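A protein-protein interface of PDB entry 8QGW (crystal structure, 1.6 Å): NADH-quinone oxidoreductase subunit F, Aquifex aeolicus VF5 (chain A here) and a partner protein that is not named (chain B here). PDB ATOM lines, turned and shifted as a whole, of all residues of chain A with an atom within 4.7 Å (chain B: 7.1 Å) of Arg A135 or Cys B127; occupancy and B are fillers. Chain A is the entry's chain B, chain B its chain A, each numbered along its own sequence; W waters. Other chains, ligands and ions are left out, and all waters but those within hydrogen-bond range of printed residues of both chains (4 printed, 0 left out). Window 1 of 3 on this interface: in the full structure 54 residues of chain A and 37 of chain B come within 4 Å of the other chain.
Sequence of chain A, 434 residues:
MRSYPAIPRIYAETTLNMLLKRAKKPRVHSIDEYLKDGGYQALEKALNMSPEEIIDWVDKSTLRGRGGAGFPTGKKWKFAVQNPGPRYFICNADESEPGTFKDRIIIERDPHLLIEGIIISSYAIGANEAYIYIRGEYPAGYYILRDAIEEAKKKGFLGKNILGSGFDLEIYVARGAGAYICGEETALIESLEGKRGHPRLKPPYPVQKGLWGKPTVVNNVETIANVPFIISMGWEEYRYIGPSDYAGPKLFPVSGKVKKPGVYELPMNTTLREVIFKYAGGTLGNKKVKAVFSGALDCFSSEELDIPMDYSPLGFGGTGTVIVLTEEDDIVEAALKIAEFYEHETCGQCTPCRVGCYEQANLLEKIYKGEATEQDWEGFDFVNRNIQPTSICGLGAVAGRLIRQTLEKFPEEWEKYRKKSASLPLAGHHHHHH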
ATOM      1  N   ALA A  93      19.438 -15.005  10.625  1.00  0.00           N
ATOM      2  CA  ALA A  93      18.773 -14.881   9.345  1.00  0.00           C
ATOM      3  C   ALA A  93      19.506 -13.866   8.467  1.00  0.00           C
ATOM      4  O   ALA A  93      18.885 -13.139   7.698  1.00  0.00           O
ATOM      5  CB  ALA A  93      17.319 -14.530   9.549  1.00  0.00           C
ATOM      6  N   ASP A  94      20.853 -13.842   8.536  1.00  0.00           N
ATOM      7  CA  ASP A  94      21.587 -12.859   7.741  1.00  0.00           C
ATOM      8  C   ASP A  94      21.794 -13.283   6.276  1.00  0.00           C
ATOM      9  O   ASP A  94      22.134 -12.437   5.450  1.00  0.00           O
ATOM     10  CB  ASP A  94      22.951 -12.495   8.347  1.00  0.00           C
ATOM     11  CG  ASP A  94      23.427 -11.141   7.823  1.00  0.00           C
ATOM     12  OD1 ASP A  94      22.711 -10.142   8.019  1.00  0.00           O
ATOM     13  OD2 ASP A  94      24.484 -11.118   7.143  1.00  0.00           O
ATOM     14  N   GLU A  95      21.634 -14.569   5.991  1.00  0.00           N
ATOM     15  CA  GLU A  95      21.770 -15.210   4.690  1.00  0.00           C
ATOM     16  C   GLU A  95      22.179 -14.259   3.566  1.00  0.00           C
ATOM     17  O   GLU A  95      21.338 -13.684   2.878  1.00  0.00           O
ATOM     18  CB  GLU A  95      20.471 -15.941   4.364  1.00  0.00           C
ATOM     19  CG  GLU A  95      20.522 -16.606   3.002  1.00  0.00           C
ATOM     20  CD  GLU A  95      19.358 -17.538   2.783  1.00  0.00           C
ATOM     21  OE1 GLU A  95      18.249 -17.005   2.588  1.00  0.00           O
ATOM     22  OE2 GLU A  95      19.578 -18.794   2.853  1.00  0.00           O
ATOM     23  N   SER A  96      23.501 -14.130   3.334  1.00  0.00           N
ATOM     24  CA  SER A  96      24.006 -13.185   2.352  1.00  0.00           C
ATOM     25  C   SER A  96      25.124 -13.780   1.488  1.00  0.00           C
ATOM     26  O   SER A  96      25.686 -13.037   0.696  1.00  0.00           O
ATOM     27  CB  SER A  96      24.493 -11.901   3.049  1.00  0.00           C
ATOM     28  OG  SER A  96      23.388 -11.132   3.490  1.00  0.00           O
ATOM     29  N   GLU A  97      25.462 -15.072   1.645  1.00  0.00           N
ATOM     30  CA  GLU A  97      26.487 -15.666   0.792  1.00  0.00           C
ATOM     31  C   GLU A  97      25.941 -15.857  -0.623  1.00  0.00           C
ATOM     32  O   GLU A  97      24.823 -16.356  -0.787  1.00  0.00           O
ATOM     33  CB  GLU A  97      26.925 -17.022   1.331  1.00  0.00           C
ATOM     34  CG  GLU A  97      28.147 -17.553   0.602  1.00  0.00           C
ATOM     35  CD  GLU A  97      28.781 -18.813   1.149  1.00  0.00           C
ATOM     36  OE1 GLU A  97      28.425 -19.257   2.286  1.00  0.00           O
ATOM     37  OE2 GLU A  97      29.648 -19.346   0.443  1.00  0.00           O
ATOM     38  N   PRO A  98      26.705 -15.501  -1.686  1.00  0.00           N
ATOM     39  CA  PRO A  98      26.265 -15.714  -3.060  1.00  0.00           C
ATOM     40  C   PRO A  98      25.745 -17.125  -3.311  1.00  0.00           C
ATOM     41  O   PRO A  98      26.364 -18.106  -2.901  1.00  0.00           O
ATOM     42  CB  PRO A  98      27.521 -15.409  -3.882  1.00  0.00           C
ATOM     43  CG  PRO A  98      28.188 -14.323  -3.067  1.00  0.00           C
ATOM     44  CD  PRO A  98      27.997 -14.793  -1.640  1.00  0.00           C
ATOM     45  N   GLY A  99      24.581 -17.189  -3.961  1.00  0.00           N
ATOM     46  CA  GLY A  99      23.937 -18.448  -4.284  1.00  0.00           C
ATOM     47  C   GLY A  99      22.948 -18.932  -3.219  1.00  0.00           C
ATOM     48  O   GLY A  99      22.210 -19.903  -3.463  1.00  0.00           O
ATOM     49  N   TYR A 133      17.977 -11.925  13.771  1.00  0.00           N
ATOM     50  CA  TYR A 133      18.753 -10.924  13.048  1.00  0.00           C
ATOM     51  C   TYR A 133      18.598 -11.228  11.558  1.00  0.00           C
ATOM     52  O   TYR A 133      19.142 -12.216  11.072  1.00  0.00           O
ATOM     53  CB  TYR A 133      20.213 -10.905  13.505  1.00  0.00           C
ATOM     54  CG  TYR A 133      21.034  -9.781  12.925  1.00  0.00           C
ATOM     55  CD1 TYR A 133      21.570  -9.842  11.643  1.00  0.00           C
ATOM     56  CD2 TYR A 133      21.210  -8.610  13.652  1.00  0.00           C
ATOM     57  CE1 TYR A 133      22.323  -8.787  11.138  1.00  0.00           C
ATOM     58  CE2 TYR A 133      21.975  -7.563  13.155  1.00  0.00           C
ATOM     59  CZ  TYR A 133      22.527  -7.649  11.894  1.00  0.00           C
ATOM     60  OH  TYR A 133      23.296  -6.595  11.398  1.00  0.00           O
ATOM     61  N   ILE A 134      17.786 -10.415  10.867  1.00  0.00           N
ATOM     62  CA  ILE A 134      17.509 -10.625   9.449  1.00  0.00           C
ATOM     63  C   ILE A 134      18.193  -9.544   8.625  1.00  0.00           C
ATOM     64  O   ILE A 134      18.127  -8.366   8.955  1.00  0.00           O
ATOM     65  CB  ILE A 134      15.989 -10.727   9.169  1.00  0.00           C
ATOM     66  CG1 ILE A 134      15.702 -11.184   7.726  1.00  0.00           C
ATOM     67  CG2 ILE A 134      15.217  -9.468   9.542  1.00  0.00           C
ATOM     68  CD1 ILE A 134      14.243 -11.496   7.449  1.00  0.00           C
ATOM     69  N   ARG A 135      18.842  -9.949   7.526  1.00  0.00           N
ATOM     70  CA  ARG A 135      19.536  -9.001   6.672  1.00  0.00           C
ATOM     71  C   ARG A 135      18.574  -7.892   6.247  1.00  0.00           C
ATOM     72  O   ARG A 135      17.360  -8.079   6.081  1.00  0.00           O
ATOM     73  CB  ARG A 135      20.169  -9.714   5.463  1.00  0.00           C
ATOM     74  CG  ARG A 135      19.167 -10.325   4.488  1.00  0.00           C
ATOM     75  CD  ARG A 135      19.838 -11.037   3.332  1.00  0.00           C
ATOM     76  NE  ARG A 135      20.564 -10.097   2.497  1.00  0.00           N
ATOM     77  CZ  ARG A 135      21.121 -10.394   1.315  1.00  0.00           C
ATOM     78  NH1 ARG A 135      21.104 -11.642   0.872  1.00  0.00           N
ATOM     79  NH2 ARG A 135      21.706  -9.429   0.623  1.00  0.00           N
ATOM     80  N   GLY A 136      19.130  -6.694   6.109  1.00  0.00           N
ATOM     81  CA  GLY A 136      18.360  -5.542   5.671  1.00  0.00           C
ATOM     82  C   GLY A 136      17.694  -5.700   4.305  1.00  0.00           C
ATOM     83  O   GLY A 136      16.666  -5.053   4.064  1.00  0.00           O
ATOM     84  N   GLU A 137      18.267  -6.533   3.432  1.00  0.00           N
ATOM     85  CA  GLU A 137      17.772  -6.686   2.062  1.00  0.00           C
ATOM     86  C   GLU A 137      16.634  -7.709   1.985  1.00  0.00           C
ATOM     87  O   GLU A 137      16.172  -8.029   0.886  1.00  0.00           O
ATOM     88  CB  GLU A 137      18.904  -7.063   1.090  1.00  0.00           C
ATOM     89  CG  GLU A 137      20.073  -6.072   1.054  1.00  0.00           C
ATOM     90  CD  GLU A 137      21.126  -6.276   2.137  1.00  0.00           C
ATOM     91  OE1 GLU A 137      20.937  -7.158   3.020  1.00  0.00           O
ATOM     92  OE2 GLU A 137      22.142  -5.555   2.092  1.00  0.00           O
ATOM     93  N   TYR A 138      16.125  -8.144   3.148  1.00  0.00           N
ATOM     94  CA  TYR A 138      14.961  -9.011   3.242  1.00  0.00           C
ATOM     95  C   TYR A 138      13.855  -8.260   3.981  1.00  0.00           C
ATOM     96  O   TYR A 138      13.401  -8.656   5.061  1.00  0.00           O
ATOM     97  CB  TYR A 138      15.271 -10.309   3.983  1.00  0.00           C
ATOM     98  CG  TYR A 138      16.058 -11.406   3.284  1.00  0.00           C
ATOM     99  CD1 TYR A 138      16.358 -11.389   1.927  1.00  0.00           C
ATOM    100  CD2 TYR A 138      16.434 -12.523   4.014  1.00  0.00           C
ATOM    101  CE1 TYR A 138      17.013 -12.454   1.322  1.00  0.00           C
ATOM    102  CE2 TYR A 138      17.091 -13.595   3.429  1.00  0.00           C
ATOM    103  CZ  TYR A 138      17.382 -13.553   2.069  1.00  0.00           C
ATOM    104  OH  TYR A 138      18.063 -14.560   1.420  1.00  0.00           O
ATOM    105  N   GLY A 176      19.674  -6.125   9.718  1.00  0.00           N
ATOM    106  CA  GLY A 176      20.963  -5.701   9.219  1.00  0.00           C
ATOM    107  C   GLY A 176      20.848  -4.505   8.288  1.00  0.00           C
ATOM    108  O   GLY A 176      19.753  -3.963   8.070  1.00  0.00           O
ATOM    109  N   HIS B  35      17.366   3.078   9.195  1.00  0.00           N
ATOM    110  CA  HIS B  35      16.502   2.665   8.095  1.00  0.00           C
ATOM    111  C   HIS B  35      15.313   3.622   7.981  1.00  0.00           C
ATOM    112  O   HIS B  35      14.932   4.023   6.889  1.00  0.00           O
ATOM    113  CB  HIS B  35      16.019   1.222   8.289  1.00  0.00           C
ATOM    114  CG  HIS B  35      16.999   0.192   7.876  1.00  0.00           C
ATOM    115  ND1 HIS B  35      17.403   0.054   6.566  1.00  0.00           N
ATOM    116  CD2 HIS B  35      17.597  -0.808   8.561  1.00  0.00           C
ATOM    117  CE1 HIS B  35      18.228  -0.973   6.475  1.00  0.00           C
ATOM    118  NE2 HIS B  35      18.353  -1.522   7.676  1.00  0.00           N
ATOM    119  N   MET B  72      23.943  -0.201   3.164  1.00  0.00           N
ATOM    120  CA  MET B  72      22.620   0.187   2.687  1.00  0.00           C
ATOM    121  C   MET B  72      22.416   1.691   2.865  1.00  0.00           C
ATOM    122  O   MET B  72      21.642   2.314   2.125  1.00  0.00           O
ATOM    123  CB  MET B  72      21.504  -0.565   3.414  1.00  0.00           C
ATOM    124  CG  MET B  72      21.367  -2.002   2.935  1.00  0.00           C
ATOM    125  SD  MET B  72      19.982  -2.915   3.661  1.00  0.00           S
ATOM    126  CE  MET B  72      18.589  -2.122   2.882  1.00  0.00           C
ATOM    127  N   CYS B  86      21.688  -6.503  -8.348  1.00  0.00           N
ATOM    128  CA  CYS B  86      22.679  -7.481  -7.950  1.00  0.00           C
ATOM    129  C   CYS B  86      23.767  -7.612  -9.015  1.00  0.00           C
ATOM    130  O   CYS B  86      23.462  -7.835 -10.186  1.00  0.00           O
ATOM    131  CB  CYS B  86      22.052  -8.840  -7.729  1.00  0.00           C
ATOM    132  SG  CYS B  86      23.272 -10.013  -7.110  1.00  0.00           S
ATOM    133  N   VAL B  87      25.040  -7.517  -8.576  1.00  0.00           N
ATOM    134  CA  VAL B  87      26.191  -7.601  -9.467  1.00  0.00           C
ATOM    135  C   VAL B  87      27.064  -8.802  -9.101  1.00  0.00           C
ATOM    136  O   VAL B  87      28.184  -8.935  -9.618  1.00  0.00           O
ATOM    137  CB  VAL B  87      27.021  -6.291  -9.486  1.00  0.00           C
ATOM    138  CG1 VAL B  87      26.212  -5.117 -10.029  1.00  0.00           C
ATOM    139  CG2 VAL B  87      27.597  -5.919  -8.134  1.00  0.00           C
ATOM    140  N   SER B  88      26.554  -9.676  -8.226  1.00  0.00           N
ATOM    141  CA  SER B  88      27.295 -10.855  -7.788  1.00  0.00           C
ATOM    142  C   SER B  88      27.230 -11.971  -8.832  1.00  0.00           C
ATOM    143  O   SER B  88      26.565 -11.841  -9.857  1.00  0.00           O
ATOM    144  CB  SER B  88      26.833 -11.326  -6.431  1.00  0.00           C
ATOM    145  OG  SER B  88      27.275 -10.437  -5.394  1.00  0.00           O
ATOM    146  N   ILE B  89      27.866 -13.108  -8.506  1.00  0.00           N
ATOM    147  CA  ILE B  89      28.178 -14.148  -9.491  1.00  0.00           C
ATOM    148  C   ILE B  89      26.962 -14.660 -10.286  1.00  0.00           C
ATOM    149  O   ILE B  89      27.029 -14.742 -11.524  1.00  0.00           O
ATOM    150  CB  ILE B  89      28.998 -15.306  -8.859  1.00  0.00           C
ATOM    151  CG1 ILE B  89      29.309 -16.419  -9.866  1.00  0.00           C
ATOM    152  CG2 ILE B  89      28.350 -15.906  -7.627  1.00  0.00           C
ATOM    153  CD1 ILE B  89      30.256 -16.030 -10.914  1.00  0.00           C
ATOM    154  N   VAL B  90      25.884 -15.072  -9.606  1.00  0.00           N
ATOM    155  CA  VAL B  90      24.811 -15.751 -10.319  1.00  0.00           C
ATOM    156  C   VAL B  90      24.078 -14.764 -11.225  1.00  0.00           C
ATOM    157  O   VAL B  90      23.860 -15.026 -12.418  1.00  0.00           O
ATOM    158  CB  VAL B  90      23.830 -16.491  -9.389  1.00  0.00           C
ATOM    159  CG1 VAL B  90      22.859 -17.342 -10.214  1.00  0.00           C
ATOM    160  CG2 VAL B  90      24.536 -17.316  -8.330  1.00  0.00           C
ATOM    161  N   CYS B  91      23.758 -13.573 -10.712  1.00  0.00           N
ATOM    162  CA  CYS B  91      23.107 -12.582 -11.556  1.00  0.00           C
ATOM    163  C   CYS B  91      24.020 -12.178 -12.719  1.00  0.00           C
ATOM    164  O   CYS B  91      23.554 -11.978 -13.845  1.00  0.00           O
ATOM    165  CB  CYS B  91      22.627 -11.406 -10.717  1.00  0.00           C
ATOM    166  SG  CYS B  91      21.311 -11.887  -9.565  1.00  0.00           S
ATOM    167  N   VAL B 125      24.655  -3.808  -5.849  1.00  0.00           N
ATOM    168  CA  VAL B 125      24.699  -4.507  -4.571  1.00  0.00           C
ATOM    169  C   VAL B 125      25.227  -5.926  -4.764  1.00  0.00           C
ATOM    170  O   VAL B 125      25.187  -6.501  -5.859  1.00  0.00           O
ATOM    171  CB  VAL B 125      23.312  -4.531  -3.884  1.00  0.00           C
ATOM    172  CG1 VAL B 125      22.838  -3.117  -3.561  1.00  0.00           C
ATOM    173  CG2 VAL B 125      22.272  -5.268  -4.702  1.00  0.00           C
ATOM    174  N   GLN B 126      25.666  -6.495  -3.645  1.00  0.00           N
ATOM    175  CA  GLN B 126      26.038  -7.897  -3.581  1.00  0.00           C
ATOM    176  C   GLN B 126      24.778  -8.768  -3.553  1.00  0.00           C
ATOM    177  O   GLN B 126      23.650  -8.294  -3.408  1.00  0.00           O
ATOM    178  CB  GLN B 126      26.947  -8.121  -2.376  1.00  0.00           C
ATOM    179  CG  GLN B 126      28.191  -7.227  -2.359  1.00  0.00           C
ATOM    180  CD  GLN B 126      29.063  -7.388  -3.572  1.00  0.00           C
ATOM    181  OE1 GLN B 126      29.684  -8.433  -3.766  1.00  0.00           O
ATOM    182  NE2 GLN B 126      29.157  -6.355  -4.398  1.00  0.00           N
ATOM    183  N   CYS B 127      24.992 -10.071  -3.675  1.00  0.00           N
ATOM    184  CA  CYS B 127      23.940 -11.078  -3.751  1.00  0.00           C
ATOM    185  C   CYS B 127      22.754 -10.748  -2.845  1.00  0.00           C
ATOM    186  O   CYS B 127      22.918 -10.649  -1.626  1.00  0.00           O
ATOM    187  CB  CYS B 127      24.482 -12.435  -3.340  1.00  0.00           C
ATOM    188  SG  CYS B 127      23.246 -13.761  -3.419  1.00  0.00           S
ATOM    189  N   LEU B 128      21.561 -10.671  -3.457  1.00  0.00           N
ATOM    190  CA  LEU B 128      20.306 -10.369  -2.774  1.00  0.00           C
ATOM    191  C   LEU B 128      19.583 -11.620  -2.273  1.00  0.00           C
ATOM    192  O   LEU B 128      18.443 -11.530  -1.811  1.00  0.00           O
ATOM    193  CB  LEU B 128      19.408  -9.598  -3.742  1.00  0.00           C
ATOM    194  CG  LEU B 128      19.830  -8.156  -3.996  1.00  0.00           C
ATOM    195  CD1 LEU B 128      19.066  -7.526  -5.157  1.00  0.00           C
ATOM    196  CD2 LEU B 128      19.633  -7.330  -2.733  1.00  0.00           C
ATOM    197  N   GLY B 129      20.220 -12.794  -2.349  1.00  0.00           N
ATOM    198  CA  GLY B 129      19.576 -14.012  -1.886  1.00  0.00           C
ATOM    199  C   GLY B 129      18.283 -14.338  -2.652  1.00  0.00           C
ATOM    200  O   GLY B 129      17.314 -14.817  -2.059  1.00  0.00           O
ATOM    201  N   ALA B 130      18.286 -14.164  -3.979  1.00  0.00           N
ATOM    202  CA  ALA B 130      17.207 -14.663  -4.835  1.00  0.00           C
ATOM    203  C   ALA B 130      17.755 -15.260  -6.135  1.00  0.00           C
ATOM    204  O   ALA B 130      17.182 -15.064  -7.222  1.00  0.00           O
ATOM    205  CB  ALA B 130      16.230 -13.546  -5.122  1.00  0.00           C
ATOM    206  N   CYS B 131      18.868 -15.994  -6.019  1.00  0.00           N
ATOM    207  CA  CYS B 131      19.747 -16.265  -7.148  1.00  0.00           C
ATOM    208  C   CYS B 131      19.082 -17.153  -8.213  1.00  0.00           C
ATOM    209  O   CYS B 131      19.434 -17.062  -9.379  1.00  0.00           O
ATOM    210  CB  CYS B 131      21.019 -16.929  -6.635  1.00  0.00           C
ATOM    211  SG  CYS B 131      21.709 -16.155  -5.139  1.00  0.00           S
HETATM  212  O   HOH W   1      22.916  -6.970  -1.006  1.00  0.00           O
HETATM  213  O   HOH W   2      25.395 -10.512  -0.282  1.00  0.00           O
HETATM  214  O   HOH W   3      16.661  -9.694  -1.202  1.00  0.00           O
HETATM  215  O   HOH W   4      22.359 -14.333  -0.277  1.00  0.00           O
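The side-chain carboxylate (OE2) of Glu A137 sits close to the side-chain sulfur (SD) of Met B72, at 3.8 Å. O of Cys B127 sits at hydrogen-bond distance from NH2 of Arg A135. A ring nitrogen (NE2) of His B35 sits at hydrogen-bond distance from the backbone carbonyl oxygen (O) of Gly A176. The side-chain sulfur (SG) of Cys B131 lies close to the backbone NH (N) of Gly A99 (3.3 Å). N of Gly A99 lies close to SG of Cys B127 (3.7 Å).
The guanidinium group (NE) of Arg A135 is in salt-bridge range of the side-chain carboxylate (OE1) of Glu A137 (3.0 Å). The backbone carbonyl oxygen (O) of Ala A93 sits at hydrogen-bond distance from the backbone NH (N) of Arg A135, at 3.2 Å. OG of Ser B88 lies within hydrogen-bond range of N of Cys B127, at 2.9 Å. N of Gly A136 lies close to O of Gly A176 (3.4 Å). The backbone carbonyl oxygen (O) of Glu A95 lies within hydrogen-bond range of the guanidinium group (NH1) of Arg A135, 2.9 Å away. The side-chain carboxylate (OE1) of Glu A95 sits at hydrogen-bond distance from the side-chain hydroxyl (OH) of Tyr A138.
Among the printed residues, pairs that only touch across the chains: Pro A98 with Ile B89 (3.9 Å), Pro A98 with Cys B127 (3.6 Å), Arg A135 with Leu B128 (3.5 Å), Arg A135 with Gly B129 (3.5 Å), Gly A136 with Met B72 (3.7 Å), Glu A137 with Leu B128 (3.9 Å), Tyr A138 with Leu B128 (3.6 Å) and Tyr A138 with Gly B129 (3.6 Å).
Arg A135 touches just these residues of chain B: Cys B127, Leu B128 and Gly B129. Of the printed residues of chain A, Cys B127 touches Pro A98, Gly A99 and Arg A135. Of the printed residues of chain B, Glu A137 touches Met B72 and Leu B128. Of the printed residues of chain B, Gly A99 touches Cys B127 (3.7 Å) and Cys B131 (3.3 Å). Ser B88 touches none of the printed residues of chain A. The nearest residue of chain B that does not touch Arg A135 is Gln B126 (4.6 Å).
Of the 15 printed residues of chain B, 7 touch a printed residue of chain A. Of the 14 printed residues of chain A, 7 touch a printed residue of chain B. Printed residues of chain A that touch a printed residue of chain B: Pro A98, Gly A99, Arg A135, Gly A136, Glu A137, Tyr A138 and Gly A176. Hydrophobic or aromatic side chains of chain A within 4 Å of the printed part of chain B: Pro A98 and Tyr A138.
Water W3 lies within hydrogen-bond range of O of Leu B128 (2.6 Å) and O of Glu A137 (2.7 Å). Water W2 lies within hydrogen-bond range of O of Ser A96 (2.7 Å) and O of Cys B127 (2.8 Å). Water W1 lies within hydrogen-bond range of O of Gln B126 (2.8 Å), NH2 of Arg A135 (3.2 Å) and OE2 of Glu A137 (3.5 Å). Water W4 lies within hydrogen-bond range of NH1 of Arg A135 (3.2 Å), O of Glu A97 (3.2 Å), N of Gly B129 (3.4 Å) and O of Glu A95 (3.4 Å).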
